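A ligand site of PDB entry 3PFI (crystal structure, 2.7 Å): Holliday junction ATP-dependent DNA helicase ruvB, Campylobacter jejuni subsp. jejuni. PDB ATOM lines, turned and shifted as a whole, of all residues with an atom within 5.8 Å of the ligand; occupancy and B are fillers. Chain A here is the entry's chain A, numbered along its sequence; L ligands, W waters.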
ATOM      1  N   LEU A  23      36.567  30.857 -22.155  1.00  0.00           N
ATOM      2  CA  LEU A  23      35.677  32.054 -22.118  1.00  0.00           C
ATOM      3  C   LEU A  23      34.204  31.624 -22.051  1.00  0.00           C
ATOM      4  O   LEU A  23      33.347  32.092 -22.805  1.00  0.00           O
ATOM      5  CB  LEU A  23      35.944  32.953 -23.327  1.00  0.00           C
ATOM      6  CG  LEU A  23      37.441  33.250 -23.512  1.00  0.00           C
ATOM      7  CD1 LEU A  23      38.185  31.955 -23.816  1.00  0.00           C
ATOM      8  CD2 LEU A  23      37.706  34.273 -24.610  1.00  0.00           C
ATOM      9  N   ARG A  24      33.948  30.688 -21.145  1.00  0.00           N
ATOM     10  CA  ARG A  24      32.621  30.177 -20.873  1.00  0.00           C
ATOM     11  C   ARG A  24      32.322  30.529 -19.417  1.00  0.00           C
ATOM     12  O   ARG A  24      33.248  30.773 -18.644  1.00  0.00           O
ATOM     13  CB  ARG A  24      32.568  28.663 -21.072  1.00  0.00           C
ATOM     14  CG  ARG A  24      33.639  27.865 -20.336  1.00  0.00           C
ATOM     15  CD  ARG A  24      33.269  26.390 -20.263  1.00  0.00           C
ATOM     16  NE  ARG A  24      33.084  25.775 -21.582  1.00  0.00           N
ATOM     17  CZ  ARG A  24      33.946  24.934 -22.164  1.00  0.00           C
ATOM     18  NH1 ARG A  24      35.067  24.573 -21.538  1.00  0.00           N
ATOM     19  NH2 ARG A  24      33.682  24.432 -23.368  1.00  0.00           N
ATOM     20  N   PRO A  25      31.037  30.576 -19.026  1.00  0.00           N
ATOM     21  CA  PRO A  25      30.728  30.927 -17.639  1.00  0.00           C
ATOM     22  C   PRO A  25      31.548  30.123 -16.621  1.00  0.00           C
ATOM     23  O   PRO A  25      31.765  28.922 -16.799  1.00  0.00           O
ATOM     24  CB  PRO A  25      29.228  30.626 -17.511  1.00  0.00           C
ATOM     25  CG  PRO A  25      28.829  29.928 -18.787  1.00  0.00           C
ATOM     26  CD  PRO A  25      29.813  30.342 -19.824  1.00  0.00           C
ATOM     27  N   TYR A  31      24.802  32.221 -14.794  1.00  0.00           N
ATOM     28  CA  TYR A  31      24.638  31.144 -15.776  1.00  0.00           C
ATOM     29  C   TYR A  31      23.267  31.265 -16.427  1.00  0.00           C
ATOM     30  O   TYR A  31      22.258  31.300 -15.720  1.00  0.00           O
ATOM     31  CB  TYR A  31      24.769  29.789 -15.094  1.00  0.00           C
ATOM     32  CG  TYR A  31      24.711  28.589 -16.018  1.00  0.00           C
ATOM     33  CD1 TYR A  31      25.876  28.046 -16.561  1.00  0.00           C
ATOM     34  CD2 TYR A  31      23.506  27.971 -16.316  1.00  0.00           C
ATOM     35  CE1 TYR A  31      25.828  26.943 -17.388  1.00  0.00           C
ATOM     36  CE2 TYR A  31      23.457  26.868 -17.143  1.00  0.00           C
ATOM     37  CZ  TYR A  31      24.623  26.353 -17.677  1.00  0.00           C
ATOM     38  OH  TYR A  31      24.575  25.250 -18.504  1.00  0.00           O
ATOM     39  N   ILE A  32      23.232  31.319 -17.764  1.00  0.00           N
ATOM     40  CA  ILE A  32      21.973  31.500 -18.480  1.00  0.00           C
ATOM     41  C   ILE A  32      21.325  30.182 -18.867  1.00  0.00           C
ATOM     42  O   ILE A  32      21.986  29.271 -19.342  1.00  0.00           O
ATOM     43  CB  ILE A  32      22.163  32.319 -19.772  1.00  0.00           C
ATOM     44  CG1 ILE A  32      22.959  33.595 -19.498  1.00  0.00           C
ATOM     45  CG2 ILE A  32      20.803  32.631 -20.397  1.00  0.00           C
ATOM     46  CD1 ILE A  32      22.308  34.520 -18.497  1.00  0.00           C
ATOM     47  N   GLY A  33      20.004  30.098 -18.668  1.00  0.00           N
ATOM     48  CA  GLY A  33      19.241  28.916 -19.014  1.00  0.00           C
ATOM     49  C   GLY A  33      19.399  27.752 -18.059  1.00  0.00           C
ATOM     50  O   GLY A  33      20.117  27.848 -17.051  1.00  0.00           O
ATOM     51  N   GLN A  34      18.720  26.654 -18.373  1.00  0.00           N
ATOM     52  CA  GLN A  34      18.729  25.449 -17.559  1.00  0.00           C
ATOM     53  C   GLN A  34      18.262  25.775 -16.149  1.00  0.00           C
ATOM     54  O   GLN A  34      18.817  25.274 -15.160  1.00  0.00           O
ATOM     55  CB  GLN A  34      20.115  24.805 -17.547  1.00  0.00           C
ATOM     56  CG  GLN A  34      20.729  24.544 -18.931  1.00  0.00           C
ATOM     57  CD  GLN A  34      19.926  23.558 -19.773  1.00  0.00           C
ATOM     58  OE1 GLN A  34      19.002  22.897 -19.291  1.00  0.00           O
ATOM     59  NE2 GLN A  34      20.294  23.441 -21.039  1.00  0.00           N
ATOM     60  N   GLY A  62      22.184  15.069 -23.231  1.00  0.00           N
ATOM     61  CA  GLY A  62      21.561  16.033 -24.123  1.00  0.00           C
ATOM     62  C   GLY A  62      22.456  16.345 -25.309  1.00  0.00           C
ATOM     63  O   GLY A  62      23.661  16.108 -25.256  1.00  0.00           O
ATOM     64  N   PRO A  63      21.857  16.891 -26.377  1.00  0.00           N
ATOM     65  CA  PRO A  63      22.535  17.236 -27.631  1.00  0.00           C
ATOM     66  C   PRO A  63      23.812  18.029 -27.434  1.00  0.00           C
ATOM     67  O   PRO A  63      23.928  18.790 -26.472  1.00  0.00           O
ATOM     68  CB  PRO A  63      21.496  18.101 -28.348  1.00  0.00           C
ATOM     69  CG  PRO A  63      20.206  17.561 -27.872  1.00  0.00           C
ATOM     70  CD  PRO A  63      20.429  17.224 -26.428  1.00  0.00           C
ATOM     71  N   ALA A  64      24.756  17.855 -28.346  1.00  0.00           N
ATOM     72  CA  ALA A  64      26.061  18.527 -28.272  1.00  0.00           C
ATOM     73  C   ALA A  64      25.944  20.037 -28.267  1.00  0.00           C
ATOM     74  O   ALA A  64      25.031  20.600 -28.882  1.00  0.00           O
ATOM     75  CB  ALA A  64      26.940  18.081 -29.428  1.00  0.00           C
ATOM     76  N   GLY A  65      26.882  20.676 -27.564  1.00  0.00           N
ATOM     77  CA  GLY A  65      26.945  22.129 -27.478  1.00  0.00           C
ATOM     78  C   GLY A  65      25.877  22.814 -26.640  1.00  0.00           C
ATOM     79  O   GLY A  65      25.656  24.020 -26.803  1.00  0.00           O
ATOM     80  N   LEU A  66      25.235  22.084 -25.747  1.00  0.00           N
ATOM     81  CA  LEU A  66      24.198  22.683 -24.901  1.00  0.00           C
ATOM     82  C   LEU A  66      24.732  23.126 -23.540  1.00  0.00           C
ATOM     83  O   LEU A  66      23.999  23.681 -22.730  1.00  0.00           O
ATOM     84  CB  LEU A  66      22.978  21.771 -24.760  1.00  0.00           C
ATOM     85  CG  LEU A  66      22.134  21.652 -26.039  1.00  0.00           C
ATOM     86  CD1 LEU A  66      20.923  20.731 -25.832  1.00  0.00           C
ATOM     87  CD2 LEU A  66      21.673  23.014 -26.518  1.00  0.00           C
ATOM     88  N   GLY A  67      26.009  22.882 -23.287  1.00  0.00           N
ATOM     89  CA  GLY A  67      26.638  23.340 -22.053  1.00  0.00           C
ATOM     90  C   GLY A  67      26.807  22.352 -20.913  1.00  0.00           C
ATOM     91  O   GLY A  67      26.766  22.744 -19.749  1.00  0.00           O
ATOM     92  N   LYS A  68      27.008  21.077 -21.228  1.00  0.00           N
ATOM     93  CA  LYS A  68      27.196  20.084 -20.180  1.00  0.00           C
ATOM     94  C   LYS A  68      28.651  20.032 -19.699  1.00  0.00           C
ATOM     95  O   LYS A  68      28.905  19.789 -18.513  1.00  0.00           O
ATOM     96  CB  LYS A  68      26.614  18.711 -20.560  1.00  0.00           C
ATOM     97  CG  LYS A  68      26.871  18.257 -21.983  1.00  0.00           C
ATOM     98  CD  LYS A  68      26.019  17.034 -22.328  1.00  0.00           C
ATOM     99  CE  LYS A  68      26.250  16.585 -23.770  1.00  0.00           C
ATOM    100  NZ  LYS A  68      25.917  17.630 -24.777  1.00  0.00           N
ATOM    101  N   THR A  69      29.601  20.288 -20.585  1.00  0.00           N
ATOM    102  CA  THR A  69      30.991  20.328 -20.167  1.00  0.00           C
ATOM    103  C   THR A  69      31.135  21.556 -19.271  1.00  0.00           C
ATOM    104  O   THR A  69      31.909  21.548 -18.305  1.00  0.00           O
ATOM    105  CB  THR A  69      31.959  20.461 -21.346  1.00  0.00           C
ATOM    106  OG1 THR A  69      31.825  19.329 -22.211  1.00  0.00           O
ATOM    107  CG2 THR A  69      33.394  20.552 -20.853  1.00  0.00           C
ATOM    108  N   THR A  70      30.385  22.601 -19.613  1.00  0.00           N
ATOM    109  CA  THR A  70      30.425  23.846 -18.847  1.00  0.00           C
ATOM    110  C   THR A  70      29.973  23.591 -17.410  1.00  0.00           C
ATOM    111  O   THR A  70      30.746  23.809 -16.468  1.00  0.00           O
ATOM    112  CB  THR A  70      29.547  24.940 -19.495  1.00  0.00           C
ATOM    113  OG1 THR A  70      30.066  25.238 -20.797  1.00  0.00           O
ATOM    114  CG2 THR A  70      29.550  26.210 -18.669  1.00  0.00           C
ATOM    115  N   LEU A  71      28.739  23.111 -17.249  1.00  0.00           N
ATOM    116  CA  LEU A  71      28.207  22.783 -15.917  1.00  0.00           C
ATOM    117  C   LEU A  71      29.192  21.968 -15.084  1.00  0.00           C
ATOM    118  O   LEU A  71      29.396  22.247 -13.899  1.00  0.00           O
ATOM    119  CB  LEU A  71      26.898  22.012 -16.042  1.00  0.00           C
ATOM    120  CG  LEU A  71      25.645  22.822 -16.344  1.00  0.00           C
ATOM    121  CD1 LEU A  71      24.513  21.933 -16.825  1.00  0.00           C
ATOM    122  CD2 LEU A  71      25.241  23.623 -15.105  1.00  0.00           C
ATOM    123  N   LEU A 181      19.740  18.212 -20.290  1.00  0.00           N
ATOM    124  CA  LEU A 181      19.732  19.607 -20.719  1.00  0.00           C
ATOM    125  C   LEU A 181      18.673  19.832 -21.778  1.00  0.00           C
ATOM    126  O   LEU A 181      18.439  18.969 -22.636  1.00  0.00           O
ATOM    127  CB  LEU A 181      21.093  20.028 -21.257  1.00  0.00           C
ATOM    128  CG  LEU A 181      22.214  20.272 -20.239  1.00  0.00           C
ATOM    129  CD1 LEU A 181      22.473  19.053 -19.385  1.00  0.00           C
ATOM    130  CD2 LEU A 181      23.482  20.700 -20.974  1.00  0.00           C
ATOM    131  N   TYR A 184      17.755  26.043 -25.640  1.00  0.00           N
ATOM    132  CA  TYR A 184      17.602  27.402 -25.151  1.00  0.00           C
ATOM    133  C   TYR A 184      16.585  28.228 -25.915  1.00  0.00           C
ATOM    134  O   TYR A 184      16.376  28.039 -27.120  1.00  0.00           O
ATOM    135  CB  TYR A 184      18.968  28.115 -25.187  1.00  0.00           C
ATOM    136  CG  TYR A 184      19.974  27.501 -24.257  1.00  0.00           C
ATOM    137  CD1 TYR A 184      20.638  26.332 -24.597  1.00  0.00           C
ATOM    138  CD2 TYR A 184      20.261  28.080 -23.033  1.00  0.00           C
ATOM    139  CE1 TYR A 184      21.556  25.761 -23.741  1.00  0.00           C
ATOM    140  CE2 TYR A 184      21.189  27.508 -22.174  1.00  0.00           C
ATOM    141  CZ  TYR A 184      21.831  26.348 -22.541  1.00  0.00           C
ATOM    142  OH  TYR A 184      22.740  25.768 -21.691  1.00  0.00           O
ATOM    143  N   ILE A 192      23.278  35.276 -23.729  1.00  0.00           N
ATOM    144  CA  ILE A 192      24.566  34.598 -23.849  1.00  0.00           C
ATOM    145  C   ILE A 192      25.465  35.326 -24.849  1.00  0.00           C
ATOM    146  O   ILE A 192      26.653  35.521 -24.602  1.00  0.00           O
ATOM    147  CB  ILE A 192      24.398  33.127 -24.264  1.00  0.00           C
ATOM    148  CG1 ILE A 192      23.699  32.345 -23.153  1.00  0.00           C
ATOM    149  CG2 ILE A 192      25.754  32.514 -24.572  1.00  0.00           C
ATOM    150  CD1 ILE A 192      23.448  30.879 -23.474  1.00  0.00           C
ATOM    151  N   PRO A 220      23.940  27.229 -27.892  1.00  0.00           N
ATOM    152  CA  PRO A 220      24.988  28.181 -27.555  1.00  0.00           C
ATOM    153  C   PRO A 220      26.228  28.109 -28.432  1.00  0.00           C
ATOM    154  O   PRO A 220      26.758  29.150 -28.814  1.00  0.00           O
ATOM    155  CB  PRO A 220      25.357  27.801 -26.115  1.00  0.00           C
ATOM    156  CG  PRO A 220      24.088  27.265 -25.543  1.00  0.00           C
ATOM    157  CD  PRO A 220      23.355  26.604 -26.685  1.00  0.00           C
ATOM    158  N   ARG A 221      26.692  26.906 -28.754  1.00  0.00           N
ATOM    159  CA  ARG A 221      27.902  26.762 -29.562  1.00  0.00           C
ATOM    160  C   ARG A 221      27.741  27.326 -30.964  1.00  0.00           C
ATOM    161  O   ARG A 221      28.619  28.030 -31.451  1.00  0.00           O
ATOM    162  CB  ARG A 221      28.332  25.301 -29.640  1.00  0.00           C
ATOM    163  CG  ARG A 221      29.541  25.060 -30.510  1.00  0.00           C
ATOM    164  CD  ARG A 221      29.915  23.608 -30.473  1.00  0.00           C
ATOM    165  NE  ARG A 221      30.404  23.218 -29.146  1.00  0.00           N
ATOM    166  CZ  ARG A 221      30.512  21.968 -28.717  1.00  0.00           C
ATOM    167  NH1 ARG A 221      30.127  20.956 -29.485  1.00  0.00           N
ATOM    168  NH2 ARG A 221      30.988  21.733 -27.494  1.00  0.00           N
ATOM    169  N   LEU A 224      27.563  31.101 -30.619  1.00  0.00           N
ATOM    170  CA  LEU A 224      28.869  31.677 -30.320  1.00  0.00           C
ATOM    171  C   LEU A 224      29.750  31.617 -31.552  1.00  0.00           C
ATOM    172  O   LEU A 224      30.634  32.449 -31.725  1.00  0.00           O
ATOM    173  CB  LEU A 224      29.553  30.945 -29.153  1.00  0.00           C
ATOM    174  CG  LEU A 224      28.930  31.189 -27.778  1.00  0.00           C
ATOM    175  CD1 LEU A 224      29.444  30.181 -26.762  1.00  0.00           C
ATOM    176  CD2 LEU A 224      29.161  32.632 -27.305  1.00  0.00           C
HETATM  177  P1  LIG L   1      28.738  20.446 -24.474  1.00  0.00           P
HETATM  178  O1  LIG L   1      29.486  20.076 -23.226  1.00  0.00           O
HETATM  179  O2  LIG L   1      29.450  20.078 -25.744  1.00  0.00           O
HETATM  180  O3  LIG L   1      27.268  20.056 -24.471  1.00  0.00           O
HETATM  181  P2  LIG L   1      29.855  22.986 -23.868  1.00  0.00           P
HETATM  182  O4  LIG L   1      29.785  22.966 -22.360  1.00  0.00           O
HETATM  183  O5  LIG L   1      31.157  22.634 -24.539  1.00  0.00           O
HETATM  184  O6  LIG L   1      28.673  22.059 -24.466  1.00  0.00           O
HETATM  185  O7  LIG L   1      29.424  24.450 -24.340  1.00  0.00           O
HETATM  186  C1  LIG L   1      29.498  24.864 -25.700  1.00  0.00           C
HETATM  187  C2  LIG L   1      29.711  26.370 -25.766  1.00  0.00           C
HETATM  188  O8  LIG L   1      28.481  27.048 -25.471  1.00  0.00           O
HETATM  189  C3  LIG L   1      30.743  26.856 -24.754  1.00  0.00           C
HETATM  190  O9  LIG L   1      31.587  27.858 -25.333  1.00  0.00           O
HETATM  191  C4  LIG L   1      29.920  27.444 -23.626  1.00  0.00           C
HETATM  192  O10 LIG L   1      30.546  28.587 -23.066  1.00  0.00           O
HETATM  193  C5  LIG L   1      28.609  27.826 -24.280  1.00  0.00           C
HETATM  194  N1  LIG L   1      27.495  27.558 -23.346  1.00  0.00           N
HETATM  195  C6  LIG L   1      26.850  26.399 -23.203  1.00  0.00           C
HETATM  196  N2  LIG L   1      25.896  26.545 -22.270  1.00  0.00           N
HETATM  197  C7  LIG L   1      25.942  27.814 -21.836  1.00  0.00           C
HETATM  198  C8  LIG L   1      25.216  28.530 -20.900  1.00  0.00           C
HETATM  199  N3  LIG L   1      24.212  27.919 -20.223  1.00  0.00           N
HETATM  200  N4  LIG L   1      25.513  29.826 -20.677  1.00  0.00           N
HETATM  201  C9  LIG L   1      26.494  30.428 -21.354  1.00  0.00           C
HETATM  202  N5  LIG L   1      27.208  29.758 -22.270  1.00  0.00           N
HETATM  203  C10 LIG L   1      26.952  28.460 -22.523  1.00  0.00           C
HETATM  204  O   HOH W   1      32.236  19.800 -25.041  1.00  0.00           O
HETATM  205  O   HOH W   2      26.048  32.007 -18.237  1.00  0.00           O
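Water W1 lies within hydrogen-bond range of O2 of the ligand (2.9 Å), OG1 of Thr 69 (2.9 Å) and NH2 of Arg 221 (3.4 Å).
Water W2 lies within hydrogen-bond range of the backbone NH (N) of Ile 32 (2.9 Å) and a nitrogen (N4) of the ligand (3.3 Å).
O of Leu 66 sits at hydrogen-bond distance from OH of Tyr 184 (2.6 Å).
OG1 of Thr 70 lies within hydrogen-bond range of NE of Arg 24 (3.2 Å).
The backbone carbonyl oxygen (O) of Pro 63 sits at hydrogen-bond distance from the side-chain amino group (NZ) of Lys 68 (2.9 Å).
The backbone carbonyl oxygen of Gly 62 sits at hydrogen-bond distance from the side-chain amino group of Lys 68 (2.8 Å).
The side-chain hydroxyl (OH) of Tyr 184 is in hydrogen-bond range of the side-chain amide nitrogen (NE2) of Gln 34 (3.4 Å).
O1 of the ligand sits at hydrogen-bond distance from N of Thr 69, 2.7 Å away.
The side-chain hydroxyl (OH) of Tyr 31 sits close to a nitrogen (N3) of the ligand (3.2 Å).
N of Gly 67 is in hydrogen-bond range of O6 of the ligand, 3.0 Å away.
O3 of the ligand is in salt-bridge range of NZ of Lys 68, 2.8 Å away.
A nitrogen (N3) of the ligand is in hydrogen-bond range of the side-chain hydroxyl of Tyr 184 (3.0 Å).
O3 of the ligand sits at hydrogen-bond distance from N of Gly 65, 3.2 Å away.
O3 of the ligand sits at hydrogen-bond distance from N of Leu 66 (3.1 Å).
The side-chain hydroxyl of Thr 69 is in hydrogen-bond range of an oxygen (O1) of the ligand, 2.7 Å away.
An oxygen (O4) of the ligand lies within hydrogen-bond range of the side-chain hydroxyl of Thr 70 (2.8 Å).
The backbone carbonyl oxygen (O) of Ile 32 is in hydrogen-bond range of a nitrogen (N3) of the ligand, at 2.7 Å.
N of Thr 70 lies within hydrogen-bond range of O4 of the ligand (2.8 Å).
NH2 of Arg 221 lies within salt-bridge range of O2 of the ligand.
O1 of the ligand sits at hydrogen-bond distance from N of Lys 68 (3.3 Å).
NH2 of Arg 24 lies within salt-bridge range of O5 of the ligand, 3.3 Å away.
Pro 25 touches the ligand (CG to C9, 3.5 Å).
Ile 192 touches the ligand.
Pro 220 touches the ligand (CB to O8, 3.3 Å).
Leu 224 touches the ligand.
Of the 23 residues printed, 15 come within 4 Å of the ligand.
The nearest printed residue that does not touch the ligand is Ala 64 (4.02 Å).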
